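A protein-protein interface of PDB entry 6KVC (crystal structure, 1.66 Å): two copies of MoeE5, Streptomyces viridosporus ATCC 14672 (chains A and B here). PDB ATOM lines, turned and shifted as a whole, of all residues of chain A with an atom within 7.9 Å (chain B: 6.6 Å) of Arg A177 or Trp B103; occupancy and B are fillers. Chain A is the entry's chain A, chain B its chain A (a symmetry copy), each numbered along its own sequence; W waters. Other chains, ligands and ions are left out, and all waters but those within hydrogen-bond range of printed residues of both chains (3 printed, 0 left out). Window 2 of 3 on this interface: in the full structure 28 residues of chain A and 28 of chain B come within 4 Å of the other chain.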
ATOM      1  N   GLN A 118       5.187   1.475  13.596  1.00  0.00           N
ATOM      2  CA  GLN A 118       4.625   2.086  14.795  1.00  0.00           C
ATOM      3  C   GLN A 118       5.558   1.918  15.999  1.00  0.00           C
ATOM      4  O   GLN A 118       5.835   2.889  16.733  1.00  0.00           O
ATOM      5  CB  GLN A 118       3.245   1.484  15.067  1.00  0.00           C
ATOM      6  CG  GLN A 118       2.683   2.005  16.430  1.00  0.00           C
ATOM      7  CD  GLN A 118       2.989   1.123  17.653  1.00  0.00           C
ATOM      8  OE1 GLN A 118       3.138  -0.094  17.540  1.00  0.00           O
ATOM      9  NE2 GLN A 118       3.097   1.772  18.857  1.00  0.00           N
ATOM     10  N   MET A 121       8.563   4.238  15.563  1.00  0.00           N
ATOM     11  CA  MET A 121       8.330   5.665  15.767  1.00  0.00           C
ATOM     12  C   MET A 121       8.133   5.955  17.237  1.00  0.00           C
ATOM     13  O   MET A 121       8.597   6.984  17.706  1.00  0.00           O
ATOM     14  CB  MET A 121       7.117   6.158  14.996  1.00  0.00           C
ATOM     15  CG  MET A 121       7.196   6.078  13.439  1.00  0.00           C
ATOM     16  SD  MET A 121       8.623   6.946  12.792  1.00  0.00           S
ATOM     17  CE  MET A 121       8.330   8.648  13.377  1.00  0.00           C
ATOM     18  N   GLU A 122       7.449   5.060  17.974  1.00  0.00           N
ATOM     19  CA  GLU A 122       7.314   5.315  19.419  1.00  0.00           C
ATOM     20  C   GLU A 122       8.687   5.371  20.079  1.00  0.00           C
ATOM     21  O   GLU A 122       8.952   6.248  20.930  1.00  0.00           O
ATOM     22  CB  GLU A 122       6.453   4.236  20.066  1.00  0.00           C
ATOM     23  CG  GLU A 122       6.272   4.420  21.596  1.00  0.00           C
ATOM     24  CD  GLU A 122       5.303   3.389  22.165  1.00  0.00           C
ATOM     25  OE1 GLU A 122       4.232   3.818  22.577  1.00  0.00           O
ATOM     26  OE2 GLU A 122       5.613   2.156  22.170  1.00  0.00           O
ATOM     27  N   VAL A 125      10.381   8.651  19.491  1.00  0.00           N
ATOM     28  CA  VAL A 125       9.904   9.691  20.418  1.00  0.00           C
ATOM     29  C   VAL A 125      10.589   9.521  21.771  1.00  0.00           C
ATOM     30  O   VAL A 125      11.066  10.493  22.371  1.00  0.00           O
ATOM     31  CB  VAL A 125       8.365   9.646  20.556  1.00  0.00           C
ATOM     32  CG1 VAL A 125       7.866  10.563  21.720  1.00  0.00           C
ATOM     33  CG2 VAL A 125       7.684  10.050  19.222  1.00  0.00           C
ATOM     34  N   GLN A 126      10.620   8.282  22.272  1.00  0.00           N
ATOM     35  CA  GLN A 126      11.195   8.012  23.599  1.00  0.00           C
ATOM     36  C   GLN A 126      12.694   8.245  23.644  1.00  0.00           C
ATOM     37  O   GLN A 126      13.228   8.700  24.669  1.00  0.00           O
ATOM     38  CB  GLN A 126      10.891   6.584  24.034  1.00  0.00           C
ATOM     39  CG  GLN A 126       9.419   6.306  24.291  1.00  0.00           C
ATOM     40  CD  GLN A 126       9.098   4.820  24.376  1.00  0.00           C
ATOM     41  OE1 GLN A 126       9.637   3.997  23.620  1.00  0.00           O
ATOM     42  NE2 GLN A 126       8.210   4.461  25.313  1.00  0.00           N
ATOM     43  N   LEU A 170       1.487   6.919   9.642  1.00  0.00           N
ATOM     44  CA  LEU A 170       1.898   6.741  11.040  1.00  0.00           C
ATOM     45  C   LEU A 170       3.061   7.642  11.391  1.00  0.00           C
ATOM     46  O   LEU A 170       3.068   8.307  12.432  1.00  0.00           O
ATOM     47  CB  LEU A 170       2.313   5.300  11.276  1.00  0.00           C
ATOM     48  CG  LEU A 170       1.208   4.370  11.630  1.00  0.00           C
ATOM     49  CD1 LEU A 170       1.860   2.943  11.573  1.00  0.00           C
ATOM     50  CD2 LEU A 170       0.691   4.785  13.049  1.00  0.00           C
ATOM     51  N   ALA A 171       4.093   7.642  10.537  1.00  0.00           N
ATOM     52  CA  ALA A 171       5.276   8.445  10.792  1.00  0.00           C
ATOM     53  C   ALA A 171       4.906   9.906  10.966  1.00  0.00           C
ATOM     54  O   ALA A 171       5.351  10.547  11.918  1.00  0.00           O
ATOM     55  CB  ALA A 171       6.273   8.273   9.653  1.00  0.00           C
ATOM     56  N   LEU A 172       4.043  10.425  10.076  1.00  0.00           N
ATOM     57  CA  LEU A 172       3.606  11.816  10.184  1.00  0.00           C
ATOM     58  C   LEU A 172       2.804  12.060  11.463  1.00  0.00           C
ATOM     59  O   LEU A 172       2.934  13.142  12.089  1.00  0.00           O
ATOM     60  CB  LEU A 172       2.804  12.183   8.935  1.00  0.00           C
ATOM     61  CG  LEU A 172       3.703  12.198   7.675  1.00  0.00           C
ATOM     62  CD1 LEU A 172       2.843  12.347   6.485  1.00  0.00           C
ATOM     63  CD2 LEU A 172       4.763  13.334   7.708  1.00  0.00           C
ATOM     64  N   ALA A 173       1.969  11.086  11.871  1.00  0.00           N
ATOM     65  CA  ALA A 173       1.200  11.281  13.104  1.00  0.00           C
ATOM     66  C   ALA A 173       2.122  11.375  14.307  1.00  0.00           C
ATOM     67  O   ALA A 173       1.865  12.152  15.233  1.00  0.00           O
ATOM     68  CB  ALA A 173       0.206  10.139  13.291  1.00  0.00           C
ATOM     69  N   PHE A 174       3.185  10.567  14.346  1.00  0.00           N
ATOM     70  CA  PHE A 174       4.120  10.692  15.462  1.00  0.00           C
ATOM     71  C   PHE A 174       4.862  12.027  15.438  1.00  0.00           C
ATOM     72  O   PHE A 174       5.044  12.678  16.495  1.00  0.00           O
ATOM     73  CB  PHE A 174       5.114   9.516  15.473  1.00  0.00           C
ATOM     74  CG  PHE A 174       4.568   8.291  16.164  1.00  0.00           C
ATOM     75  CD1 PHE A 174       3.824   7.374  15.443  1.00  0.00           C
ATOM     76  CD2 PHE A 174       4.726   8.097  17.545  1.00  0.00           C
ATOM     77  CE1 PHE A 174       3.278   6.233  16.051  1.00  0.00           C
ATOM     78  CE2 PHE A 174       4.198   6.934  18.153  1.00  0.00           C
ATOM     79  CZ  PHE A 174       3.492   6.009  17.402  1.00  0.00           C
ATOM     80  N   ALA A 175       5.238  12.499  14.242  1.00  0.00           N
ATOM     81  CA  ALA A 175       5.917  13.788  14.165  1.00  0.00           C
ATOM     82  C   ALA A 175       5.021  14.940  14.611  1.00  0.00           C
ATOM     83  O   ALA A 175       5.530  15.943  15.129  1.00  0.00           O
ATOM     84  CB  ALA A 175       6.415  14.044  12.737  1.00  0.00           C
ATOM     85  N   ALA A 176       3.699  14.815  14.444  1.00  0.00           N
ATOM     86  CA  ALA A 176       2.757  15.848  14.875  1.00  0.00           C
ATOM     87  C   ALA A 176       2.404  15.830  16.357  1.00  0.00           C
ATOM     88  O   ALA A 176       1.718  16.766  16.817  1.00  0.00           O
ATOM     89  CB  ALA A 176       1.446  15.704  14.084  1.00  0.00           C
ATOM     90  N   ARG A 177       2.841  14.826  17.113  1.00  0.00           N
ATOM     91  CA  ARG A 177       2.577  14.798  18.551  1.00  0.00           C
ATOM     92  C   ARG A 177       3.179  16.032  19.242  1.00  0.00           C
ATOM     93  O   ARG A 177       4.311  16.441  18.956  1.00  0.00           O
ATOM     94  CB  ARG A 177       3.219  13.544  19.164  1.00  0.00           C
ATOM     95  CG  ARG A 177       2.546  12.229  18.764  1.00  0.00           C
ATOM     96  CD  ARG A 177       3.369  11.085  19.309  1.00  0.00           C
ATOM     97  NE  ARG A 177       3.458  11.129  20.798  1.00  0.00           N
ATOM     98  CZ  ARG A 177       2.743  10.362  21.633  1.00  0.00           C
ATOM     99  NH1 ARG A 177       1.851   9.501  21.210  1.00  0.00           N
ATOM    100  NH2 ARG A 177       2.895  10.505  22.950  1.00  0.00           N
ATOM    101  N   GLY A 178       2.414  16.615  20.170  1.00  0.00           N
ATOM    102  CA  GLY A 178       2.944  17.764  20.893  1.00  0.00           C
ATOM    103  C   GLY A 178       4.181  17.489  21.739  1.00  0.00           C
ATOM    104  O   GLY A 178       4.904  18.427  22.094  1.00  0.00           O
ATOM    105  N   ASP A 179       4.438  16.236  22.104  1.00  0.00           N
ATOM    106  CA  ASP A 179       5.555  15.890  22.979  1.00  0.00           C
ATOM    107  C   ASP A 179       6.801  15.473  22.233  1.00  0.00           C
ATOM    108  O   ASP A 179       7.754  15.000  22.857  1.00  0.00           O
ATOM    109  CB  ASP A 179       5.147  14.785  23.969  1.00  0.00           C
ATOM    110  CG  ASP A 179       4.807  13.456  23.298  1.00  0.00           C
ATOM    111  OD1 ASP A 179       4.623  13.434  22.056  1.00  0.00           O
ATOM    112  OD2 ASP A 179       4.716  12.428  24.010  1.00  0.00           O
ATOM    113  N   ALA A 180       6.791  15.584  20.916  1.00  0.00           N
ATOM    114  CA  ALA A 180       7.867  15.057  20.093  1.00  0.00           C
ATOM    115  C   ALA A 180       8.563  16.257  19.480  1.00  0.00           C
ATOM    116  O   ALA A 180       7.895  17.219  19.098  1.00  0.00           O
ATOM    117  CB  ALA A 180       7.327  14.108  19.020  1.00  0.00           C
ATOM    118  N   GLU A 181       9.894  16.246  19.493  1.00  0.00           N
ATOM    119  CA  GLU A 181      10.688  17.181  18.704  1.00  0.00           C
ATOM    120  C   GLU A 181      11.278  16.319  17.606  1.00  0.00           C
ATOM    121  O   GLU A 181      12.423  15.908  17.664  1.00  0.00           O
ATOM    122  CB  GLU A 181      11.777  17.876  19.516  1.00  0.00           C
ATOM    123  CG  GLU A 181      11.226  18.868  20.529  1.00  0.00           C
ATOM    124  CD  GLU A 181      10.400  19.970  19.879  1.00  0.00           C
ATOM    125  OE1 GLU A 181      10.780  20.445  18.780  1.00  0.00           O
ATOM    126  OE2 GLU A 181       9.363  20.353  20.469  1.00  0.00           O
ATOM    127  N   LEU A 182      10.443  16.006  16.627  1.00  0.00           N
ATOM    128  CA  LEU A 182      10.729  14.958  15.657  1.00  0.00           C
ATOM    129  C   LEU A 182      10.197  15.433  14.323  1.00  0.00           C
ATOM    130  O   LEU A 182       9.035  15.860  14.262  1.00  0.00           O
ATOM    131  CB  LEU A 182      10.007  13.688  16.122  1.00  0.00           C
ATOM    132  CG  LEU A 182      10.007  12.498  15.191  1.00  0.00           C
ATOM    133  CD1 LEU A 182      11.450  12.129  15.070  1.00  0.00           C
ATOM    134  CD2 LEU A 182       9.230  11.397  15.865  1.00  0.00           C
ATOM    135  N   GLY B  98     -12.045   3.368  19.565  1.00  0.00           N
ATOM    136  CA  GLY B  98     -11.562   4.486  20.403  1.00  0.00           C
ATOM    137  C   GLY B  98     -10.287   5.102  19.871  1.00  0.00           C
ATOM    138  O   GLY B  98      -9.301   4.406  19.599  1.00  0.00           O
ATOM    139  N   VAL B  99     -10.277   6.434  19.791  1.00  0.00           N
ATOM    140  CA  VAL B  99      -9.077   7.149  19.373  1.00  0.00           C
ATOM    141  C   VAL B  99      -7.917   6.922  20.357  1.00  0.00           C
ATOM    142  O   VAL B  99      -6.777   6.627  19.970  1.00  0.00           O
ATOM    143  CB  VAL B  99      -9.391   8.657  19.251  1.00  0.00           C
ATOM    144  CG1 VAL B  99      -8.103   9.473  19.118  1.00  0.00           C
ATOM    145  CG2 VAL B  99     -10.358   8.916  18.082  1.00  0.00           C
ATOM    146  N   ARG B 100      -8.164   7.142  21.643  1.00  0.00           N
ATOM    147  CA  ARG B 100      -7.058   7.328  22.573  1.00  0.00           C
ATOM    148  C   ARG B 100      -6.309   6.035  22.925  1.00  0.00           C
ATOM    149  O   ARG B 100      -5.062   6.074  23.007  1.00  0.00           O
ATOM    150  CB  ARG B 100      -7.609   8.056  23.793  1.00  0.00           C
ATOM    151  CG  ARG B 100      -7.877   9.518  23.398  1.00  0.00           C
ATOM    152  CD  ARG B 100      -8.651  10.319  24.466  1.00  0.00           C
ATOM    153  NE  ARG B 100     -10.004   9.822  24.663  1.00  0.00           N
ATOM    154  CZ  ARG B 100     -11.040  10.132  23.888  1.00  0.00           C
ATOM    155  NH1 ARG B 100     -10.871  10.957  22.849  1.00  0.00           N
ATOM    156  NH2 ARG B 100     -12.231   9.602  24.117  1.00  0.00           N
ATOM    157  N   PRO B 101      -6.977   4.883  23.095  1.00  0.00           N
ATOM    158  CA  PRO B 101      -6.228   3.650  23.369  1.00  0.00           C
ATOM    159  C   PRO B 101      -5.375   3.191  22.206  1.00  0.00           C
ATOM    160  O   PRO B 101      -4.558   2.292  22.393  1.00  0.00           O
ATOM    161  CB  PRO B 101      -7.324   2.615  23.672  1.00  0.00           C
ATOM    162  CG  PRO B 101      -8.505   3.420  24.122  1.00  0.00           C
ATOM    163  CD  PRO B 101      -8.425   4.644  23.201  1.00  0.00           C
ATOM    164  N   SER B 102      -5.548   3.756  21.008  1.00  0.00           N
ATOM    165  CA  SER B 102      -4.868   3.171  19.865  1.00  0.00           C
ATOM    166  C   SER B 102      -3.354   3.331  19.944  1.00  0.00           C
ATOM    167  O   SER B 102      -2.641   2.584  19.283  1.00  0.00           O
ATOM    168  CB  SER B 102      -5.415   3.783  18.539  1.00  0.00           C
ATOM    169  OG  SER B 102      -5.049   5.172  18.475  1.00  0.00           O
ATOM    170  N   TRP B 103      -2.840   4.311  20.708  1.00  0.00           N
ATOM    171  CA  TRP B 103      -1.390   4.440  20.834  1.00  0.00           C
ATOM    172  C   TRP B 103      -0.777   3.251  21.576  1.00  0.00           C
ATOM    173  O   TRP B 103       0.367   2.889  21.309  1.00  0.00           O
ATOM    174  CB  TRP B 103      -1.045   5.704  21.625  1.00  0.00           C
ATOM    175  CG  TRP B 103      -1.446   7.008  21.005  1.00  0.00           C
ATOM    176  CD1 TRP B 103      -2.460   7.805  21.391  1.00  0.00           C
ATOM    177  CD2 TRP B 103      -0.767   7.679  19.951  1.00  0.00           C
ATOM    178  NE1 TRP B 103      -2.495   8.974  20.627  1.00  0.00           N
ATOM    179  CE2 TRP B 103      -1.435   8.917  19.748  1.00  0.00           C
ATOM    180  CE3 TRP B 103       0.345   7.351  19.153  1.00  0.00           C
ATOM    181  CZ2 TRP B 103      -1.052   9.825  18.760  1.00  0.00           C
ATOM    182  CZ3 TRP B 103       0.758   8.289  18.166  1.00  0.00           C
ATOM    183  CH2 TRP B 103       0.052   9.512  17.992  1.00  0.00           C
ATOM    184  N   THR B 104      -1.481   2.695  22.557  1.00  0.00           N
ATOM    185  CA  THR B 104      -0.892   1.682  23.418  1.00  0.00           C
ATOM    186  C   THR B 104      -1.466   0.286  23.190  1.00  0.00           C
ATOM    187  O   THR B 104      -1.056  -0.673  23.860  1.00  0.00           O
ATOM    188  CB  THR B 104      -1.038   2.162  24.889  1.00  0.00           C
ATOM    189  OG1 THR B 104      -2.428   2.355  25.209  1.00  0.00           O
ATOM    190  CG2 THR B 104      -0.299   3.482  25.067  1.00  0.00           C
ATOM    191  N   GLN B 105      -2.369   0.118  22.220  1.00  0.00           N
ATOM    192  CA  GLN B 105      -2.994  -1.155  21.899  1.00  0.00           C
ATOM    193  C   GLN B 105      -2.901  -1.419  20.399  1.00  0.00           C
ATOM    194  O   GLN B 105      -3.812  -1.981  19.776  1.00  0.00           O
ATOM    195  CB  GLN B 105      -4.450  -1.170  22.366  1.00  0.00           C
ATOM    196  CG  GLN B 105      -4.598  -1.049  23.872  1.00  0.00           C
ATOM    197  CD  GLN B 105      -6.055  -0.843  24.315  1.00  0.00           C
ATOM    198  OE1 GLN B 105      -6.990  -1.145  23.586  1.00  0.00           O
ATOM    199  NE2 GLN B 105      -6.240  -0.333  25.539  1.00  0.00           N
ATOM    200  N   PHE B 106      -1.796  -0.980  19.794  1.00  0.00           N
ATOM    201  CA  PHE B 106      -1.760  -0.950  18.328  1.00  0.00           C
ATOM    202  C   PHE B 106      -1.840  -2.330  17.688  1.00  0.00           C
ATOM    203  O   PHE B 106      -2.561  -2.471  16.695  1.00  0.00           O
ATOM    204  CB  PHE B 106      -0.525  -0.195  17.825  1.00  0.00           C
ATOM    205  CG  PHE B 106      -0.644   0.182  16.372  1.00  0.00           C
ATOM    206  CD1 PHE B 106      -1.747   0.906  15.940  1.00  0.00           C
ATOM    207  CD2 PHE B 106       0.309  -0.266  15.431  1.00  0.00           C
ATOM    208  CE1 PHE B 106      -1.884   1.258  14.558  1.00  0.00           C
ATOM    209  CE2 PHE B 106       0.174   0.074  14.070  1.00  0.00           C
ATOM    210  CZ  PHE B 106      -0.923   0.841  13.642  1.00  0.00           C
ATOM    211  N   TYR B 109      -5.504  -3.027  17.477  1.00  0.00           N
ATOM    212  CA  TYR B 109      -6.170  -2.173  16.495  1.00  0.00           C
ATOM    213  C   TYR B 109      -5.842  -2.617  15.074  1.00  0.00           C
ATOM    214  O   TYR B 109      -6.710  -2.583  14.204  1.00  0.00           O
ATOM    215  CB  TYR B 109      -5.742  -0.712  16.698  1.00  0.00           C
ATOM    216  CG  TYR B 109      -6.577   0.017  17.708  1.00  0.00           C
ATOM    217  CD1 TYR B 109      -6.462  -0.285  19.090  1.00  0.00           C
ATOM    218  CD2 TYR B 109      -7.496   0.992  17.311  1.00  0.00           C
ATOM    219  CE1 TYR B 109      -7.223   0.382  20.027  1.00  0.00           C
ATOM    220  CE2 TYR B 109      -8.276   1.669  18.252  1.00  0.00           C
ATOM    221  CZ  TYR B 109      -8.148   1.343  19.584  1.00  0.00           C
ATOM    222  OH  TYR B 109      -8.919   1.984  20.525  1.00  0.00           O
ATOM    223  N   LEU B 157      -4.113  11.885  12.889  1.00  0.00           N
ATOM    224  CA  LEU B 157      -3.275  12.290  14.013  1.00  0.00           C
ATOM    225  C   LEU B 157      -3.130  11.176  15.051  1.00  0.00           C
ATOM    226  O   LEU B 157      -2.336  11.326  15.987  1.00  0.00           O
ATOM    227  CB  LEU B 157      -3.866  13.521  14.721  1.00  0.00           C
ATOM    228  CG  LEU B 157      -3.780  14.835  13.950  1.00  0.00           C
ATOM    229  CD1 LEU B 157      -4.078  16.008  14.892  1.00  0.00           C
ATOM    230  CD2 LEU B 157      -2.407  14.978  13.390  1.00  0.00           C
ATOM    231  N   SER B 158      -3.849  10.064  14.886  1.00  0.00           N
ATOM    232  CA  SER B 158      -3.772   8.956  15.836  1.00  0.00           C
ATOM    233  C   SER B 158      -3.550   7.662  15.082  1.00  0.00           C
ATOM    234  O   SER B 158      -3.917   7.533  13.902  1.00  0.00           O
ATOM    235  CB  SER B 158      -5.055   8.823  16.686  1.00  0.00           C
ATOM    236  OG  SER B 158      -6.170   8.613  15.821  1.00  0.00           O
ATOM    237  N   PRO B 159      -3.008   6.649  15.743  1.00  0.00           N
ATOM    238  CA  PRO B 159      -2.935   5.327  15.077  1.00  0.00           C
ATOM    239  C   PRO B 159      -4.297   4.771  14.733  1.00  0.00           C
ATOM    240  O   PRO B 159      -4.425   4.108  13.697  1.00  0.00           O
ATOM    241  CB  PRO B 159      -2.186   4.450  16.101  1.00  0.00           C
ATOM    242  CG  PRO B 159      -1.338   5.488  16.860  1.00  0.00           C
ATOM    243  CD  PRO B 159      -2.257   6.689  17.010  1.00  0.00           C
ATOM    244  N   TYR B 160      -5.335   5.069  15.525  1.00  0.00           N
ATOM    245  CA  TYR B 160      -6.692   4.671  15.160  1.00  0.00           C
ATOM    246  C   TYR B 160      -7.081   5.229  13.795  1.00  0.00           C
ATOM    247  O   TYR B 160      -7.578   4.494  12.937  1.00  0.00           O
ATOM    248  CB  TYR B 160      -7.693   5.160  16.221  1.00  0.00           C
ATOM    249  CG  TYR B 160      -9.119   5.078  15.766  1.00  0.00           C
ATOM    250  CD1 TYR B 160      -9.769   3.849  15.618  1.00  0.00           C
ATOM    251  CD2 TYR B 160      -9.844   6.241  15.502  1.00  0.00           C
ATOM    252  CE1 TYR B 160     -11.098   3.764  15.170  1.00  0.00           C
ATOM    253  CE2 TYR B 160     -11.200   6.182  15.067  1.00  0.00           C
ATOM    254  CZ  TYR B 160     -11.800   4.955  14.914  1.00  0.00           C
ATOM    255  OH  TYR B 160     -13.107   4.914  14.540  1.00  0.00           O
ATOM    256  N   ARG B 285      -5.367  15.042  25.530  1.00  0.00           N
ATOM    257  CA  ARG B 285      -4.782  13.760  25.178  1.00  0.00           C
ATOM    258  C   ARG B 285      -4.228  13.853  23.764  1.00  0.00           C
ATOM    259  O   ARG B 285      -4.924  14.304  22.843  1.00  0.00           O
ATOM    260  CB  ARG B 285      -5.805  12.624  25.252  1.00  0.00           C
ATOM    261  CG  ARG B 285      -6.481  12.447  26.635  1.00  0.00           C
ATOM    262  CD  ARG B 285      -5.559  12.571  27.808  1.00  0.00           C
ATOM    263  NE  ARG B 285      -6.006  11.813  28.992  1.00  0.00           N
ATOM    264  CZ  ARG B 285      -6.270  12.353  30.185  1.00  0.00           C
ATOM    265  NH1 ARG B 285      -6.194  13.660  30.361  1.00  0.00           N
ATOM    266  NH2 ARG B 285      -6.647  11.561  31.185  1.00  0.00           N
ATOM    267  N   ILE B 286      -2.959  13.477  23.615  1.00  0.00           N
ATOM    268  CA  ILE B 286      -2.329  13.443  22.299  1.00  0.00           C
ATOM    269  C   ILE B 286      -3.091  12.481  21.401  1.00  0.00           C
ATOM    270  O   ILE B 286      -3.470  11.375  21.800  1.00  0.00           O
ATOM    271  CB  ILE B 286      -0.844  13.077  22.454  1.00  0.00           C
ATOM    272  CG1 ILE B 286      -0.087  14.247  23.101  1.00  0.00           C
ATOM    273  CG2 ILE B 286      -0.198  12.824  21.146  1.00  0.00           C
ATOM    274  CD1 ILE B 286       1.356  13.921  23.464  1.00  0.00           C
ATOM    275  N   GLY B 287      -3.357  12.938  20.163  1.00  0.00           N
ATOM    276  CA  GLY B 287      -4.138  12.183  19.193  1.00  0.00           C
ATOM    277  C   GLY B 287      -5.529  12.743  19.009  1.00  0.00           C
ATOM    278  O   GLY B 287      -6.170  12.467  17.990  1.00  0.00           O
ATOM    279  N   ASP B 288      -6.030  13.497  19.990  1.00  0.00           N
ATOM    280  CA  ASP B 288      -7.358  14.108  19.855  1.00  0.00           C
ATOM    281  C   ASP B 288      -7.254  15.320  18.939  1.00  0.00           C
ATOM    282  O   ASP B 288      -6.500  16.262  19.247  1.00  0.00           O
ATOM    283  CB  ASP B 288      -7.893  14.574  21.216  1.00  0.00           C
ATOM    284  CG  ASP B 288      -8.502  13.452  22.055  1.00  0.00           C
ATOM    285  OD1 ASP B 288      -8.741  12.346  21.575  1.00  0.00           O
ATOM    286  OD2 ASP B 288      -8.793  13.694  23.266  1.00  0.00           O
HETATM  287  O   HOH W   1       2.660   1.344  21.789  1.00  0.00           O
HETATM  288  O   HOH W   2      -0.429  13.142  16.634  1.00  0.00           O
HETATM  289  O   HOH W   3       1.921   4.239  19.480  1.00  0.00           O
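Printed residues of chain B within 4 Å of Ala A173: Leu B157. Printed residues of chain B within 4 Å of Phe A174: Trp B103. Of the printed residues of chain B, Ala A176 touches Leu B157 (3.98 Å). Arg A177 touches just these residues of chain B: Trp B103 and Ile B286. Trp B103 touches just these residues of chain A: Gln A118, Phe A174 and Arg A177. Of the printed residues of chain A, Leu B157 touches Ala A173 (3.9 Å) and Ala A176 (3.98 Å). Printed residues of chain A within 4 Å of Ile B286: Arg A177 and Asp A179. The nearest printed residue of chain B that does not touch Phe A174 is Pro B159 (4.7 Å).
The guanidinium group (NH2) of Arg A177 is in salt-bridge range of the side-chain carboxylate (OD2) of Asp A179, at 2.9 Å. The backbone carbonyl oxygen of Ile B286 sits at hydrogen-bond distance from the indole nitrogen of Trp B103 (2.8 Å).
No position is printed for both chains.
Water W2 lies within hydrogen-bond range of O of Leu B157 (2.7 Å) and O of Ala A173 (2.9 Å). Water W3 bridges the backbone carbonyl oxygen of Trp B103 (2.8 Å) and the side-chain amide nitrogen of Gln A118 (2.8 Å). Water W1 lies within hydrogen-bond range of the backbone carbonyl oxygen (O) of Trp B103 (2.8 Å), the side-chain amide nitrogen (NE2) of Gln A118 (3.0 Å) and the side-chain carboxylate (OE1) of Glu A122 (3.0 Å).
Of the 18 printed residues of chain A, 6 touch a printed residue of chain B. Hydrophobic or aromatic side chains of chain B that line the printed part of chain A: Trp B103, Phe B106, Leu B157 and Ile B286. Among the printed residues, 8 pairs touch across the chains.
O of Trp B103 touches NE2 of Gln A118, at 3.8 Å. Gln A118 touches Phe B106. CB of Ala A173 touches O of Leu B157, at 3.9 Å. Phe A174 touches Trp B103 (CZ to CZ3, 3.6 Å). Leu B157 touches Ala A176 (CD2 to CB, 3.98 Å). Trp B103 touches Arg A177. CG of Arg A177 touches CG2 of Ile B286, at 3.7 Å. Asp A179 touches Ile B286 (CG to CD1, 3.5 Å).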
